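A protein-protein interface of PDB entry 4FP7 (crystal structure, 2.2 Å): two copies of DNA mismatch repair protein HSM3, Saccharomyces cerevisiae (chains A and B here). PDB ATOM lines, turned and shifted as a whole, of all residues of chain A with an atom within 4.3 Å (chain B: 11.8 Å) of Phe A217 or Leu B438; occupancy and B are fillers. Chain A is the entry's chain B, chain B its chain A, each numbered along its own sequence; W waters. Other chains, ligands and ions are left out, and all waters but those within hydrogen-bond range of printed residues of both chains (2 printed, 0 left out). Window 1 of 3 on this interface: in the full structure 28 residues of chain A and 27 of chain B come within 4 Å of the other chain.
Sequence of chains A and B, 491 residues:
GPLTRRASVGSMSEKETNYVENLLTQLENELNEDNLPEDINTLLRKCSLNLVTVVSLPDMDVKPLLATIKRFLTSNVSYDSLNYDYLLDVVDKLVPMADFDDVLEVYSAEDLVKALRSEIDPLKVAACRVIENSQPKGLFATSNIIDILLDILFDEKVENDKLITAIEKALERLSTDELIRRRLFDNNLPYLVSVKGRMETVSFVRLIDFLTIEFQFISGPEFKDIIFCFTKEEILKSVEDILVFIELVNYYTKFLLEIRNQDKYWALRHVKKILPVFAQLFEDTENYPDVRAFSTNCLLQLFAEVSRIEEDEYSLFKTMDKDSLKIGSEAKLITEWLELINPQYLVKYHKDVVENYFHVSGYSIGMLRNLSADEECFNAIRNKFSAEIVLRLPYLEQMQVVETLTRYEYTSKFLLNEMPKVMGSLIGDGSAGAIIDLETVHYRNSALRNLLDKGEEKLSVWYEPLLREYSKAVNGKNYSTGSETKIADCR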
ATOM      1  N   GLU A 172     -12.476 -21.332 -24.625  1.00  0.00           N
ATOM      2  CA  GLU A 172     -11.243 -20.604 -24.337  1.00  0.00           C
ATOM      3  C   GLU A 172     -10.992 -20.462 -22.830  1.00  0.00           C
ATOM      4  O   GLU A 172      -9.892 -20.727 -22.358  1.00  0.00           O
ATOM      5  CB  GLU A 172     -11.307 -19.224 -24.954  1.00  0.00           C
ATOM      6  CG  GLU A 172     -10.037 -18.408 -24.747  1.00  0.00           C
ATOM      7  CD  GLU A 172     -10.010 -17.166 -25.613  1.00  0.00           C
ATOM      8  OE1 GLU A 172     -11.095 -16.586 -25.857  1.00  0.00           O
ATOM      9  OE2 GLU A 172      -8.908 -16.780 -26.057  1.00  0.00           O
ATOM     10  N   SER A 175     -10.140 -23.848 -21.115  1.00  0.00           N
ATOM     11  CA  SER A 175      -9.077 -24.646 -21.729  1.00  0.00           C
ATOM     12  C   SER A 175      -7.755 -24.497 -21.004  1.00  0.00           C
ATOM     13  O   SER A 175      -6.800 -25.169 -21.344  1.00  0.00           O
ATOM     14  CB  SER A 175      -8.896 -24.317 -23.222  1.00  0.00           C
ATOM     15  OG  SER A 175      -9.939 -24.907 -23.985  1.00  0.00           O
ATOM     16  N   THR A 176      -7.708 -23.605 -20.021  1.00  0.00           N
ATOM     17  CA  THR A 176      -6.560 -23.513 -19.123  1.00  0.00           C
ATOM     18  C   THR A 176      -6.473 -24.773 -18.279  1.00  0.00           C
ATOM     19  O   THR A 176      -5.424 -25.105 -17.738  1.00  0.00           O
ATOM     20  CB  THR A 176      -6.685 -22.339 -18.144  1.00  0.00           C
ATOM     21  OG1 THR A 176      -7.857 -22.512 -17.337  1.00  0.00           O
ATOM     22  CG2 THR A 176      -6.748 -21.029 -18.884  1.00  0.00           C
ATOM     23  N   ARG A 181      -8.699 -29.926 -21.683  1.00  0.00           N
ATOM     24  CA  ARG A 181      -7.904 -30.147 -22.882  1.00  0.00           C
ATOM     25  C   ARG A 181      -7.868 -31.630 -23.282  1.00  0.00           C
ATOM     26  O   ARG A 181      -7.864 -31.945 -24.470  1.00  0.00           O
ATOM     27  CB  ARG A 181      -6.494 -29.562 -22.733  1.00  0.00           C
ATOM     28  CG  ARG A 181      -6.509 -28.052 -22.499  1.00  0.00           C
ATOM     29  CD  ARG A 181      -5.203 -27.446 -22.857  1.00  0.00           C
ATOM     30  NE  ARG A 181      -4.142 -28.025 -22.056  1.00  0.00           N
ATOM     31  CZ  ARG A 181      -3.863 -27.668 -20.810  1.00  0.00           C
ATOM     32  NH1 ARG A 181      -4.563 -26.720 -20.195  1.00  0.00           N
ATOM     33  NH2 ARG A 181      -2.872 -28.255 -20.174  1.00  0.00           N
ATOM     34  N   ILE A 213      -6.593 -20.496 -30.857  1.00  0.00           N
ATOM     35  CA  ILE A 213      -6.820 -20.256 -29.438  1.00  0.00           C
ATOM     36  C   ILE A 213      -6.202 -21.388 -28.615  1.00  0.00           C
ATOM     37  O   ILE A 213      -5.546 -21.145 -27.607  1.00  0.00           O
ATOM     38  CB  ILE A 213      -8.322 -20.204 -29.122  1.00  0.00           C
ATOM     39  CG1 ILE A 213      -8.961 -18.980 -29.754  1.00  0.00           C
ATOM     40  CG2 ILE A 213      -8.579 -20.188 -27.610  1.00  0.00           C
ATOM     41  CD1 ILE A 213     -10.480 -19.190 -30.016  1.00  0.00           C
ATOM     42  N   GLU A 214      -6.411 -22.631 -29.046  1.00  0.00           N
ATOM     43  CA  GLU A 214      -6.050 -23.768 -28.206  1.00  0.00           C
ATOM     44  C   GLU A 214      -4.559 -23.935 -28.103  1.00  0.00           C
ATOM     45  O   GLU A 214      -4.063 -24.330 -27.062  1.00  0.00           O
ATOM     46  CB  GLU A 214      -6.708 -25.063 -28.681  1.00  0.00           C
ATOM     47  CG  GLU A 214      -8.189 -25.103 -28.409  1.00  0.00           C
ATOM     48  CD  GLU A 214      -8.520 -25.165 -26.918  1.00  0.00           C
ATOM     49  OE1 GLU A 214      -7.714 -25.677 -26.108  1.00  0.00           O
ATOM     50  OE2 GLU A 214      -9.609 -24.708 -26.565  1.00  0.00           O
ATOM     51  N   PHE A 215      -3.825 -23.578 -29.146  1.00  0.00           N
ATOM     52  CA  PHE A 215      -2.389 -23.813 -29.112  1.00  0.00           C
ATOM     53  C   PHE A 215      -1.696 -23.007 -28.000  1.00  0.00           C
ATOM     54  O   PHE A 215      -0.585 -23.347 -27.574  1.00  0.00           O
ATOM     55  CB  PHE A 215      -1.740 -23.539 -30.465  1.00  0.00           C
ATOM     56  CG  PHE A 215      -0.245 -23.720 -30.454  1.00  0.00           C
ATOM     57  CD1 PHE A 215       0.321 -24.995 -30.279  1.00  0.00           C
ATOM     58  CD2 PHE A 215       0.601 -22.623 -30.601  1.00  0.00           C
ATOM     59  CE1 PHE A 215       1.722 -25.173 -30.244  1.00  0.00           C
ATOM     60  CE2 PHE A 215       2.000 -22.789 -30.563  1.00  0.00           C
ATOM     61  CZ  PHE A 215       2.557 -24.075 -30.392  1.00  0.00           C
ATOM     62  N   GLN A 216      -2.364 -21.954 -27.539  1.00  0.00           N
ATOM     63  CA  GLN A 216      -1.889 -21.118 -26.444  1.00  0.00           C
ATOM     64  C   GLN A 216      -1.718 -21.883 -25.170  1.00  0.00           C
ATOM     65  O   GLN A 216      -0.916 -21.503 -24.339  1.00  0.00           O
ATOM     66  CB  GLN A 216      -2.895 -20.018 -26.127  1.00  0.00           C
ATOM     67  CG  GLN A 216      -2.857 -18.824 -27.030  1.00  0.00           C
ATOM     68  CD  GLN A 216      -4.070 -17.935 -26.812  1.00  0.00           C
ATOM     69  OE1 GLN A 216      -5.191 -18.417 -26.537  1.00  0.00           O
ATOM     70  NE2 GLN A 216      -3.855 -16.629 -26.909  1.00  0.00           N
ATOM     71  N   PHE A 217      -2.510 -22.934 -25.001  1.00  0.00           N
ATOM     72  CA  PHE A 217      -2.574 -23.653 -23.743  1.00  0.00           C
ATOM     73  C   PHE A 217      -1.943 -25.035 -23.815  1.00  0.00           C
ATOM     74  O   PHE A 217      -1.971 -25.769 -22.834  1.00  0.00           O
ATOM     75  CB  PHE A 217      -4.028 -23.844 -23.321  1.00  0.00           C
ATOM     76  CG  PHE A 217      -4.849 -22.598 -23.382  1.00  0.00           C
ATOM     77  CD1 PHE A 217      -4.577 -21.533 -22.548  1.00  0.00           C
ATOM     78  CD2 PHE A 217      -5.914 -22.501 -24.265  1.00  0.00           C
ATOM     79  CE1 PHE A 217      -5.349 -20.382 -22.598  1.00  0.00           C
ATOM     80  CE2 PHE A 217      -6.679 -21.355 -24.329  1.00  0.00           C
ATOM     81  CZ  PHE A 217      -6.402 -20.296 -23.493  1.00  0.00           C
ATOM     82  N   ILE A 218      -1.397 -25.396 -24.969  1.00  0.00           N
ATOM     83  CA  ILE A 218      -0.966 -26.759 -25.211  1.00  0.00           C
ATOM     84  C   ILE A 218       0.521 -26.920 -24.900  1.00  0.00           C
ATOM     85  O   ILE A 218       1.349 -26.191 -25.430  1.00  0.00           O
ATOM     86  CB  ILE A 218      -1.236 -27.162 -26.671  1.00  0.00           C
ATOM     87  CG1 ILE A 218      -2.706 -27.510 -26.854  1.00  0.00           C
ATOM     88  CG2 ILE A 218      -0.389 -28.370 -27.070  1.00  0.00           C
ATOM     89  CD1 ILE A 218      -3.081 -28.909 -26.379  1.00  0.00           C
ATOM     90  N   SER A 219       0.850 -27.875 -24.033  1.00  0.00           N
ATOM     91  CA  SER A 219       2.250 -28.154 -23.691  1.00  0.00           C
ATOM     92  C   SER A 219       2.822 -29.154 -24.687  1.00  0.00           C
ATOM     93  O   SER A 219       2.062 -29.817 -25.388  1.00  0.00           O
ATOM     94  CB  SER A 219       2.339 -28.755 -22.297  1.00  0.00           C
ATOM     95  OG  SER A 219       1.662 -30.008 -22.263  1.00  0.00           O
ATOM     96  N   GLU A 222       1.325 -32.715 -24.842  1.00  0.00           N
ATOM     97  CA  GLU A 222      -0.057 -32.825 -25.340  1.00  0.00           C
ATOM     98  C   GLU A 222      -0.174 -32.590 -26.849  1.00  0.00           C
ATOM     99  O   GLU A 222      -1.192 -32.916 -27.448  1.00  0.00           O
ATOM    100  CB  GLU A 222      -0.968 -31.787 -24.676  1.00  0.00           C
ATOM    101  CG  GLU A 222      -1.059 -31.809 -23.164  1.00  0.00           C
ATOM    102  CD  GLU A 222      -1.732 -30.524 -22.629  1.00  0.00           C
ATOM    103  OE1 GLU A 222      -1.018 -29.538 -22.307  1.00  0.00           O
ATOM    104  OE2 GLU A 222      -2.978 -30.506 -22.544  1.00  0.00           O
ATOM    105  N   ARG B 369       4.807 -10.622  -4.891  1.00  0.00           N
ATOM    106  CA  ARG B 369       5.011  -9.927  -6.173  1.00  0.00           C
ATOM    107  C   ARG B 369       5.031  -8.421  -6.012  1.00  0.00           C
ATOM    108  O   ARG B 369       5.652  -7.730  -6.793  1.00  0.00           O
ATOM    109  CB  ARG B 369       3.918 -10.283  -7.178  1.00  0.00           C
ATOM    110  CG  ARG B 369       4.127 -11.645  -7.798  1.00  0.00           C
ATOM    111  CD  ARG B 369       2.990 -12.055  -8.711  1.00  0.00           C
ATOM    112  NE  ARG B 369       3.206 -13.413  -9.217  1.00  0.00           N
ATOM    113  CZ  ARG B 369       2.240 -14.284  -9.511  1.00  0.00           C
ATOM    114  NH1 ARG B 369       0.959 -13.958  -9.370  1.00  0.00           N
ATOM    115  NH2 ARG B 369       2.554 -15.491  -9.966  1.00  0.00           N
ATOM    116  N   TYR B 395       5.008 -27.628  -6.461  1.00  0.00           N
ATOM    117  CA  TYR B 395       5.927 -27.135  -7.483  1.00  0.00           C
ATOM    118  C   TYR B 395       5.426 -25.882  -8.204  1.00  0.00           C
ATOM    119  O   TYR B 395       6.193 -24.939  -8.352  1.00  0.00           O
ATOM    120  CB  TYR B 395       6.251 -28.224  -8.508  1.00  0.00           C
ATOM    121  CG  TYR B 395       7.583 -28.001  -9.177  1.00  0.00           C
ATOM    122  CD1 TYR B 395       8.764 -28.009  -8.433  1.00  0.00           C
ATOM    123  CD2 TYR B 395       7.669 -27.779 -10.539  1.00  0.00           C
ATOM    124  CE1 TYR B 395       9.987 -27.796  -9.025  1.00  0.00           C
ATOM    125  CE2 TYR B 395       8.905 -27.575 -11.154  1.00  0.00           C
ATOM    126  CZ  TYR B 395      10.059 -27.587 -10.389  1.00  0.00           C
ATOM    127  OH  TYR B 395      11.282 -27.387 -10.989  1.00  0.00           O
ATOM    128  N   LEU B 396       4.169 -25.873  -8.659  1.00  0.00           N
ATOM    129  CA  LEU B 396       3.554 -24.645  -9.205  1.00  0.00           C
ATOM    130  C   LEU B 396       3.774 -23.414  -8.296  1.00  0.00           C
ATOM    131  O   LEU B 396       4.165 -22.381  -8.785  1.00  0.00           O
ATOM    132  CB  LEU B 396       2.044 -24.809  -9.480  1.00  0.00           C
ATOM    133  CG  LEU B 396       1.333 -23.471  -9.794  1.00  0.00           C
ATOM    134  CD1 LEU B 396       1.862 -22.847 -11.083  1.00  0.00           C
ATOM    135  CD2 LEU B 396      -0.189 -23.617  -9.868  1.00  0.00           C
ATOM    136  N   GLU B 397       3.551 -23.546  -6.991  1.00  0.00           N
ATOM    137  CA  GLU B 397       3.719 -22.421  -6.058  1.00  0.00           C
ATOM    138  C   GLU B 397       5.184 -22.067  -5.899  1.00  0.00           C
ATOM    139  O   GLU B 397       5.528 -20.870  -5.808  1.00  0.00           O
ATOM    140  CB  GLU B 397       3.103 -22.724  -4.681  1.00  0.00           C
ATOM    141  CG  GLU B 397       1.589 -22.517  -4.590  1.00  0.00           C
ATOM    142  CD  GLU B 397       0.760 -23.537  -5.401  1.00  0.00           C
ATOM    143  OE1 GLU B 397       1.287 -24.617  -5.765  1.00  0.00           O
ATOM    144  OE2 GLU B 397      -0.432 -23.245  -5.684  1.00  0.00           O
ATOM    145  N   MET B 399       7.432 -22.466  -8.246  1.00  0.00           N
ATOM    146  CA  MET B 399       7.824 -21.775  -9.484  1.00  0.00           C
ATOM    147  C   MET B 399       7.340 -20.318  -9.514  1.00  0.00           C
ATOM    148  O   MET B 399       8.015 -19.443 -10.049  1.00  0.00           O
ATOM    149  CB  MET B 399       7.321 -22.548 -10.701  1.00  0.00           C
ATOM    150  CG  MET B 399       8.039 -23.883 -10.897  1.00  0.00           C
ATOM    151  SD  MET B 399       9.837 -23.662 -10.981  1.00  0.00           S
ATOM    152  CE  MET B 399      10.341 -23.999  -9.297  1.00  0.00           C
ATOM    153  N   GLN B 400       6.180 -20.054  -8.924  1.00  0.00           N
ATOM    154  CA  GLN B 400       5.668 -18.678  -8.833  1.00  0.00           C
ATOM    155  C   GLN B 400       6.566 -17.816  -7.949  1.00  0.00           C
ATOM    156  O   GLN B 400       6.924 -16.698  -8.307  1.00  0.00           O
ATOM    157  CB  GLN B 400       4.239 -18.676  -8.296  1.00  0.00           C
ATOM    158  CG  GLN B 400       3.196 -19.042  -9.358  1.00  0.00           C
ATOM    159  CD  GLN B 400       1.874 -19.534  -8.758  1.00  0.00           C
ATOM    160  OE1 GLN B 400       1.803 -19.899  -7.580  1.00  0.00           O
ATOM    161  NE2 GLN B 400       0.831 -19.570  -9.577  1.00  0.00           N
ATOM    162  N   GLU B 403      10.043 -17.493  -9.693  1.00  0.00           N
ATOM    163  CA  GLU B 403       9.968 -16.590 -10.852  1.00  0.00           C
ATOM    164  C   GLU B 403       9.951 -15.136 -10.369  1.00  0.00           C
ATOM    165  O   GLU B 403      10.570 -14.261 -10.980  1.00  0.00           O
ATOM    166  CB  GLU B 403       8.714 -16.884 -11.696  1.00  0.00           C
ATOM    167  CG  GLU B 403       8.652 -16.138 -13.014  1.00  0.00           C
ATOM    168  CD  GLU B 403       8.010 -14.737 -12.900  1.00  0.00           C
ATOM    169  OE1 GLU B 403       7.295 -14.466 -11.912  1.00  0.00           O
ATOM    170  OE2 GLU B 403       8.218 -13.901 -13.806  1.00  0.00           O
ATOM    171  N   ALA B 432      11.072 -32.479 -15.807  1.00  0.00           N
ATOM    172  CA  ALA B 432      10.414 -31.213 -16.173  1.00  0.00           C
ATOM    173  C   ALA B 432       9.748 -31.224 -17.562  1.00  0.00           C
ATOM    174  O   ALA B 432       8.824 -30.446 -17.824  1.00  0.00           O
ATOM    175  CB  ALA B 432      11.417 -30.058 -16.077  1.00  0.00           C
ATOM    176  N   GLY B 433      10.224 -32.093 -18.449  1.00  0.00           N
ATOM    177  CA  GLY B 433       9.645 -32.229 -19.776  1.00  0.00           C
ATOM    178  C   GLY B 433       8.300 -32.934 -19.735  1.00  0.00           C
ATOM    179  O   GLY B 433       7.532 -32.889 -20.695  1.00  0.00           O
ATOM    180  N   ALA B 434       8.011 -33.585 -18.615  1.00  0.00           N
ATOM    181  CA  ALA B 434       6.721 -34.225 -18.411  1.00  0.00           C
ATOM    182  C   ALA B 434       5.648 -33.217 -17.982  1.00  0.00           C
ATOM    183  O   ALA B 434       4.455 -33.528 -18.025  1.00  0.00           O
ATOM    184  CB  ALA B 434       6.846 -35.330 -17.374  1.00  0.00           C
ATOM    185  N   ILE B 435       6.061 -32.013 -17.579  1.00  0.00           N
ATOM    186  CA  ILE B 435       5.097 -31.039 -17.057  1.00  0.00           C
ATOM    187  C   ILE B 435       4.103 -30.554 -18.133  1.00  0.00           C
ATOM    188  O   ILE B 435       4.508 -30.033 -19.179  1.00  0.00           O
ATOM    189  CB  ILE B 435       5.802 -29.808 -16.461  1.00  0.00           C
ATOM    190  CG1 ILE B 435       6.791 -30.234 -15.370  1.00  0.00           C
ATOM    191  CG2 ILE B 435       4.764 -28.846 -15.882  1.00  0.00           C
ATOM    192  CD1 ILE B 435       7.622 -29.091 -14.850  1.00  0.00           C
ATOM    193  N   ILE B 436       2.808 -30.717 -17.883  1.00  0.00           N
ATOM    194  CA  ILE B 436       1.818 -30.177 -18.820  1.00  0.00           C
ATOM    195  C   ILE B 436       1.053 -29.003 -18.219  1.00  0.00           C
ATOM    196  O   ILE B 436       0.363 -28.284 -18.945  1.00  0.00           O
ATOM    197  CB  ILE B 436       0.809 -31.236 -19.325  1.00  0.00           C
ATOM    198  CG1 ILE B 436      -0.138 -31.669 -18.193  1.00  0.00           C
ATOM    199  CG2 ILE B 436       1.543 -32.440 -19.920  1.00  0.00           C
ATOM    200  CD1 ILE B 436      -1.358 -32.448 -18.681  1.00  0.00           C
ATOM    201  N   ASP B 437       1.169 -28.808 -16.904  1.00  0.00           N
ATOM    202  CA  ASP B 437       0.430 -27.740 -16.233  1.00  0.00           C
ATOM    203  C   ASP B 437       0.859 -26.385 -16.792  1.00  0.00           C
ATOM    204  O   ASP B 437       2.046 -26.039 -16.808  1.00  0.00           O
ATOM    205  CB  ASP B 437       0.605 -27.790 -14.706  1.00  0.00           C
ATOM    206  CG  ASP B 437      -0.155 -26.662 -13.997  1.00  0.00           C
ATOM    207  OD1 ASP B 437      -1.400 -26.757 -13.899  1.00  0.00           O
ATOM    208  OD2 ASP B 437       0.483 -25.675 -13.552  1.00  0.00           O
ATOM    209  N   LEU B 438      -0.129 -25.637 -17.272  1.00  0.00           N
ATOM    210  CA  LEU B 438       0.093 -24.388 -17.997  1.00  0.00           C
ATOM    211  C   LEU B 438       0.956 -23.385 -17.224  1.00  0.00           C
ATOM    212  O   LEU B 438       1.932 -22.823 -17.748  1.00  0.00           O
ATOM    213  CB  LEU B 438      -1.272 -23.751 -18.317  1.00  0.00           C
ATOM    214  CG  LEU B 438      -1.286 -22.387 -19.028  1.00  0.00           C
ATOM    215  CD1 LEU B 438      -0.715 -22.527 -20.439  1.00  0.00           C
ATOM    216  CD2 LEU B 438      -2.697 -21.782 -19.070  1.00  0.00           C
ATOM    217  N   GLU B 439       0.563 -23.133 -15.983  1.00  0.00           N
ATOM    218  CA  GLU B 439       1.212 -22.110 -15.186  1.00  0.00           C
ATOM    219  C   GLU B 439       2.622 -22.541 -14.769  1.00  0.00           C
ATOM    220  O   GLU B 439       3.567 -21.760 -14.875  1.00  0.00           O
ATOM    221  CB  GLU B 439       0.368 -21.774 -13.956  1.00  0.00           C
ATOM    222  CG  GLU B 439      -0.703 -20.723 -14.188  1.00  0.00           C
ATOM    223  CD  GLU B 439      -1.452 -20.391 -12.908  1.00  0.00           C
ATOM    224  OE1 GLU B 439      -2.333 -21.197 -12.523  1.00  0.00           O
ATOM    225  OE2 GLU B 439      -1.150 -19.342 -12.285  1.00  0.00           O
ATOM    226  N   THR B 440       2.762 -23.784 -14.313  1.00  0.00           N
ATOM    227  CA  THR B 440       4.057 -24.279 -13.875  1.00  0.00           C
ATOM    228  C   THR B 440       5.082 -24.069 -14.976  1.00  0.00           C
ATOM    229  O   THR B 440       6.139 -23.493 -14.740  1.00  0.00           O
ATOM    230  CB  THR B 440       4.021 -25.770 -13.504  1.00  0.00           C
ATOM    231  OG1 THR B 440       3.047 -25.987 -12.484  1.00  0.00           O
ATOM    232  CG2 THR B 440       5.351 -26.202 -12.970  1.00  0.00           C
ATOM    233  N   VAL B 441       4.761 -24.508 -16.186  1.00  0.00           N
ATOM    234  CA  VAL B 441       5.707 -24.369 -17.287  1.00  0.00           C
ATOM    235  C   VAL B 441       5.990 -22.909 -17.563  1.00  0.00           C
ATOM    236  O   VAL B 441       7.147 -22.537 -17.812  1.00  0.00           O
ATOM    237  CB  VAL B 441       5.231 -25.084 -18.583  1.00  0.00           C
ATOM    238  CG1 VAL B 441       6.066 -24.643 -19.810  1.00  0.00           C
ATOM    239  CG2 VAL B 441       5.308 -26.599 -18.405  1.00  0.00           C
ATOM    240  N   HIS B 442       4.948 -22.075 -17.499  1.00  0.00           N
ATOM    241  CA  HIS B 442       5.110 -20.646 -17.765  1.00  0.00           C
ATOM    242  C   HIS B 442       6.047 -19.975 -16.752  1.00  0.00           C
ATOM    243  O   HIS B 442       6.952 -19.232 -17.128  1.00  0.00           O
ATOM    244  CB  HIS B 442       3.756 -19.923 -17.763  1.00  0.00           C
ATOM    245  CG  HIS B 442       3.872 -18.432 -17.885  1.00  0.00           C
ATOM    246  ND1 HIS B 442       4.172 -17.803 -19.076  1.00  0.00           N
ATOM    247  CD2 HIS B 442       3.748 -17.445 -16.962  1.00  0.00           C
ATOM    248  CE1 HIS B 442       4.221 -16.495 -18.883  1.00  0.00           C
ATOM    249  NE2 HIS B 442       3.967 -16.251 -17.607  1.00  0.00           N
ATOM    250  N   TYR B 443       5.819 -20.216 -15.465  1.00  0.00           N
ATOM    251  CA  TYR B 443       6.671 -19.609 -14.439  1.00  0.00           C
ATOM    252  C   TYR B 443       8.088 -20.213 -14.376  1.00  0.00           C
ATOM    253  O   TYR B 443       9.048 -19.479 -14.194  1.00  0.00           O
ATOM    254  CB  TYR B 443       5.983 -19.645 -13.074  1.00  0.00           C
ATOM    255  CG  TYR B 443       4.823 -18.689 -13.020  1.00  0.00           C
ATOM    256  CD1 TYR B 443       5.038 -17.324 -12.981  1.00  0.00           C
ATOM    257  CD2 TYR B 443       3.511 -19.152 -13.027  1.00  0.00           C
ATOM    258  CE1 TYR B 443       3.978 -16.435 -12.944  1.00  0.00           C
ATOM    259  CE2 TYR B 443       2.453 -18.285 -12.991  1.00  0.00           C
ATOM    260  CZ  TYR B 443       2.686 -16.926 -12.951  1.00  0.00           C
ATOM    261  OH  TYR B 443       1.627 -16.050 -12.914  1.00  0.00           O
ATOM    262  N   ARG B 444       8.213 -21.525 -14.561  1.00  0.00           N
ATOM    263  CA  ARG B 444       9.530 -22.158 -14.588  1.00  0.00           C
ATOM    264  C   ARG B 444      10.379 -21.598 -15.729  1.00  0.00           C
ATOM    265  O   ARG B 444      11.507 -21.136 -15.518  1.00  0.00           O
ATOM    266  CB  ARG B 444       9.417 -23.678 -14.691  1.00  0.00           C
ATOM    267  CG  ARG B 444      10.766 -24.376 -14.590  1.00  0.00           C
ATOM    268  CD  ARG B 444      10.661 -25.836 -14.218  1.00  0.00           C
ATOM    269  NE  ARG B 444      11.988 -26.442 -14.099  1.00  0.00           N
ATOM    270  CZ  ARG B 444      12.699 -26.943 -15.118  1.00  0.00           C
ATOM    271  NH1 ARG B 444      12.210 -26.953 -16.361  1.00  0.00           N
ATOM    272  NH2 ARG B 444      13.910 -27.456 -14.894  1.00  0.00           N
ATOM    273  N   ASN B 445       9.819 -21.581 -16.928  1.00  0.00           N
ATOM    274  CA  ASN B 445      10.536 -21.049 -18.067  1.00  0.00           C
ATOM    275  C   ASN B 445      10.868 -19.579 -17.922  1.00  0.00           C
ATOM    276  O   ASN B 445      11.971 -19.149 -18.333  1.00  0.00           O
ATOM    277  CB  ASN B 445       9.740 -21.296 -19.356  1.00  0.00           C
ATOM    278  CG  ASN B 445       9.663 -22.763 -19.714  1.00  0.00           C
ATOM    279  OD1 ASN B 445      10.013 -23.641 -18.909  1.00  0.00           O
ATOM    280  ND2 ASN B 445       9.185 -23.047 -20.921  1.00  0.00           N
ATOM    281  N   SER B 446       9.952 -18.801 -17.327  1.00  0.00           N
ATOM    282  CA  SER B 446      10.245 -17.380 -17.087  1.00  0.00           C
ATOM    283  C   SER B 446      11.397 -17.222 -16.095  1.00  0.00           C
ATOM    284  O   SER B 446      12.257 -16.344 -16.262  1.00  0.00           O
ATOM    285  CB  SER B 446       9.022 -16.606 -16.548  1.00  0.00           C
ATOM    286  OG  SER B 446       7.998 -16.474 -17.513  1.00  0.00           O
ATOM    287  N   ALA B 447      11.383 -18.049 -15.047  1.00  0.00           N
ATOM    288  CA  ALA B 447      12.442 -18.005 -14.037  1.00  0.00           C
ATOM    289  C   ALA B 447      13.785 -18.334 -14.681  1.00  0.00           C
ATOM    290  O   ALA B 447      14.756 -17.594 -14.531  1.00  0.00           O
ATOM    291  CB  ALA B 447      12.139 -18.962 -12.884  1.00  0.00           C
ATOM    292  N   ALA B 473      13.692 -27.220 -22.107  1.00  0.00           N
ATOM    293  CA  ALA B 473      12.281 -26.865 -21.923  1.00  0.00           C
ATOM    294  C   ALA B 473      11.653 -26.312 -23.212  1.00  0.00           C
ATOM    295  O   ALA B 473      10.515 -26.633 -23.536  1.00  0.00           O
ATOM    296  CB  ALA B 473      12.107 -25.862 -20.769  1.00  0.00           C
HETATM  297  O   HOH W   1      -2.942 -26.391 -17.290  1.00  0.00           O
HETATM  298  O   HOH W   2       0.227 -26.132 -20.784  1.00  0.00           O
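No position is printed for both chains.
Of the 4 pairs that touch across the chains among the printed residues, none has its exchanged pair printed and touching as well.
Hydrophobic or aromatic side chains of chain A that line the printed part of chain B: Phe A217.
Of the 24 printed residues of chain B, 2 touch a printed residue of chain A.
Hydrophobic or aromatic side chains of chain B that line the printed part of chain A: Ile B436 and Leu B438.
Among the printed residues, 4 pairs touch across the chains.
No residue of chain B comes within 4 Å of Glu A172.
No residue of chain B comes within 4 Å of Thr A176.
Printed residues of chain B within 4 Å of Arg A181: Ile B436.
No residue of chain B comes within 4 Å of Ile A213.
No residue of chain B comes within 4 Å of Glu A214.
Phe A215 touches none of the printed residues of chain B.
Of the printed residues of chain B, Phe A217 touches Leu B438 (3.95 Å).
Of the printed residues of chain B, Ser A219 touches Ile B436.
Printed residues of chain B within 4 Å of Glu A222: Ile B436 (3.8 Å).
Of the printed residues of chain A, Ile B436 touches Arg A181, Ser A219 and Glu A222.
Asp B437 touches none of the printed residues of chain A.
Of chain A, only Phe A217 (3.95 Å) comes within 4 Å of Leu B438.
The nearest residue of chain B that does not touch Phe A217 is Ile B436 (5.2 Å).
The nearest residue of chain A that does not touch Leu B438 is Gln A216 (4.04 Å).
O of Ile B436 lies within hydrogen-bond range of NH2 of Arg A181 (3.5 Å).
The guanidinium group of Arg A181 is in salt-bridge range of the side-chain carboxylate of Glu A222 (2.8 Å).
The backbone carbonyl oxygen of Ser A175 is in hydrogen-bond range of the guanidinium group of Arg A181 (3.0 Å).
The backbone carbonyl oxygen (O) of Thr A176 lies within hydrogen-bond range of the guanidinium group (NH1) of Arg A181 (3.1 Å).
NE of Arg A181 is in hydrogen-bond range of O of Phe A217 (3.2 Å).
OG of Ser A219 lies within hydrogen-bond range of OE1 of Glu A222 (2.7 Å).
Water W1 lies within hydrogen-bond range of O of Thr A176, N of Leu B438 and NH1 of Arg A181.
Water W2 bridges the backbone carbonyl oxygen (O) of Ile B436 (2.8 Å) and the backbone carbonyl oxygen (O) of Phe A217 (3.0 Å).
Phe A217 touches Leu B438.
Ser A219 touches Ile B436.
Glu A222 touches Ile B436 (OE1 to O, 3.8 Å).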
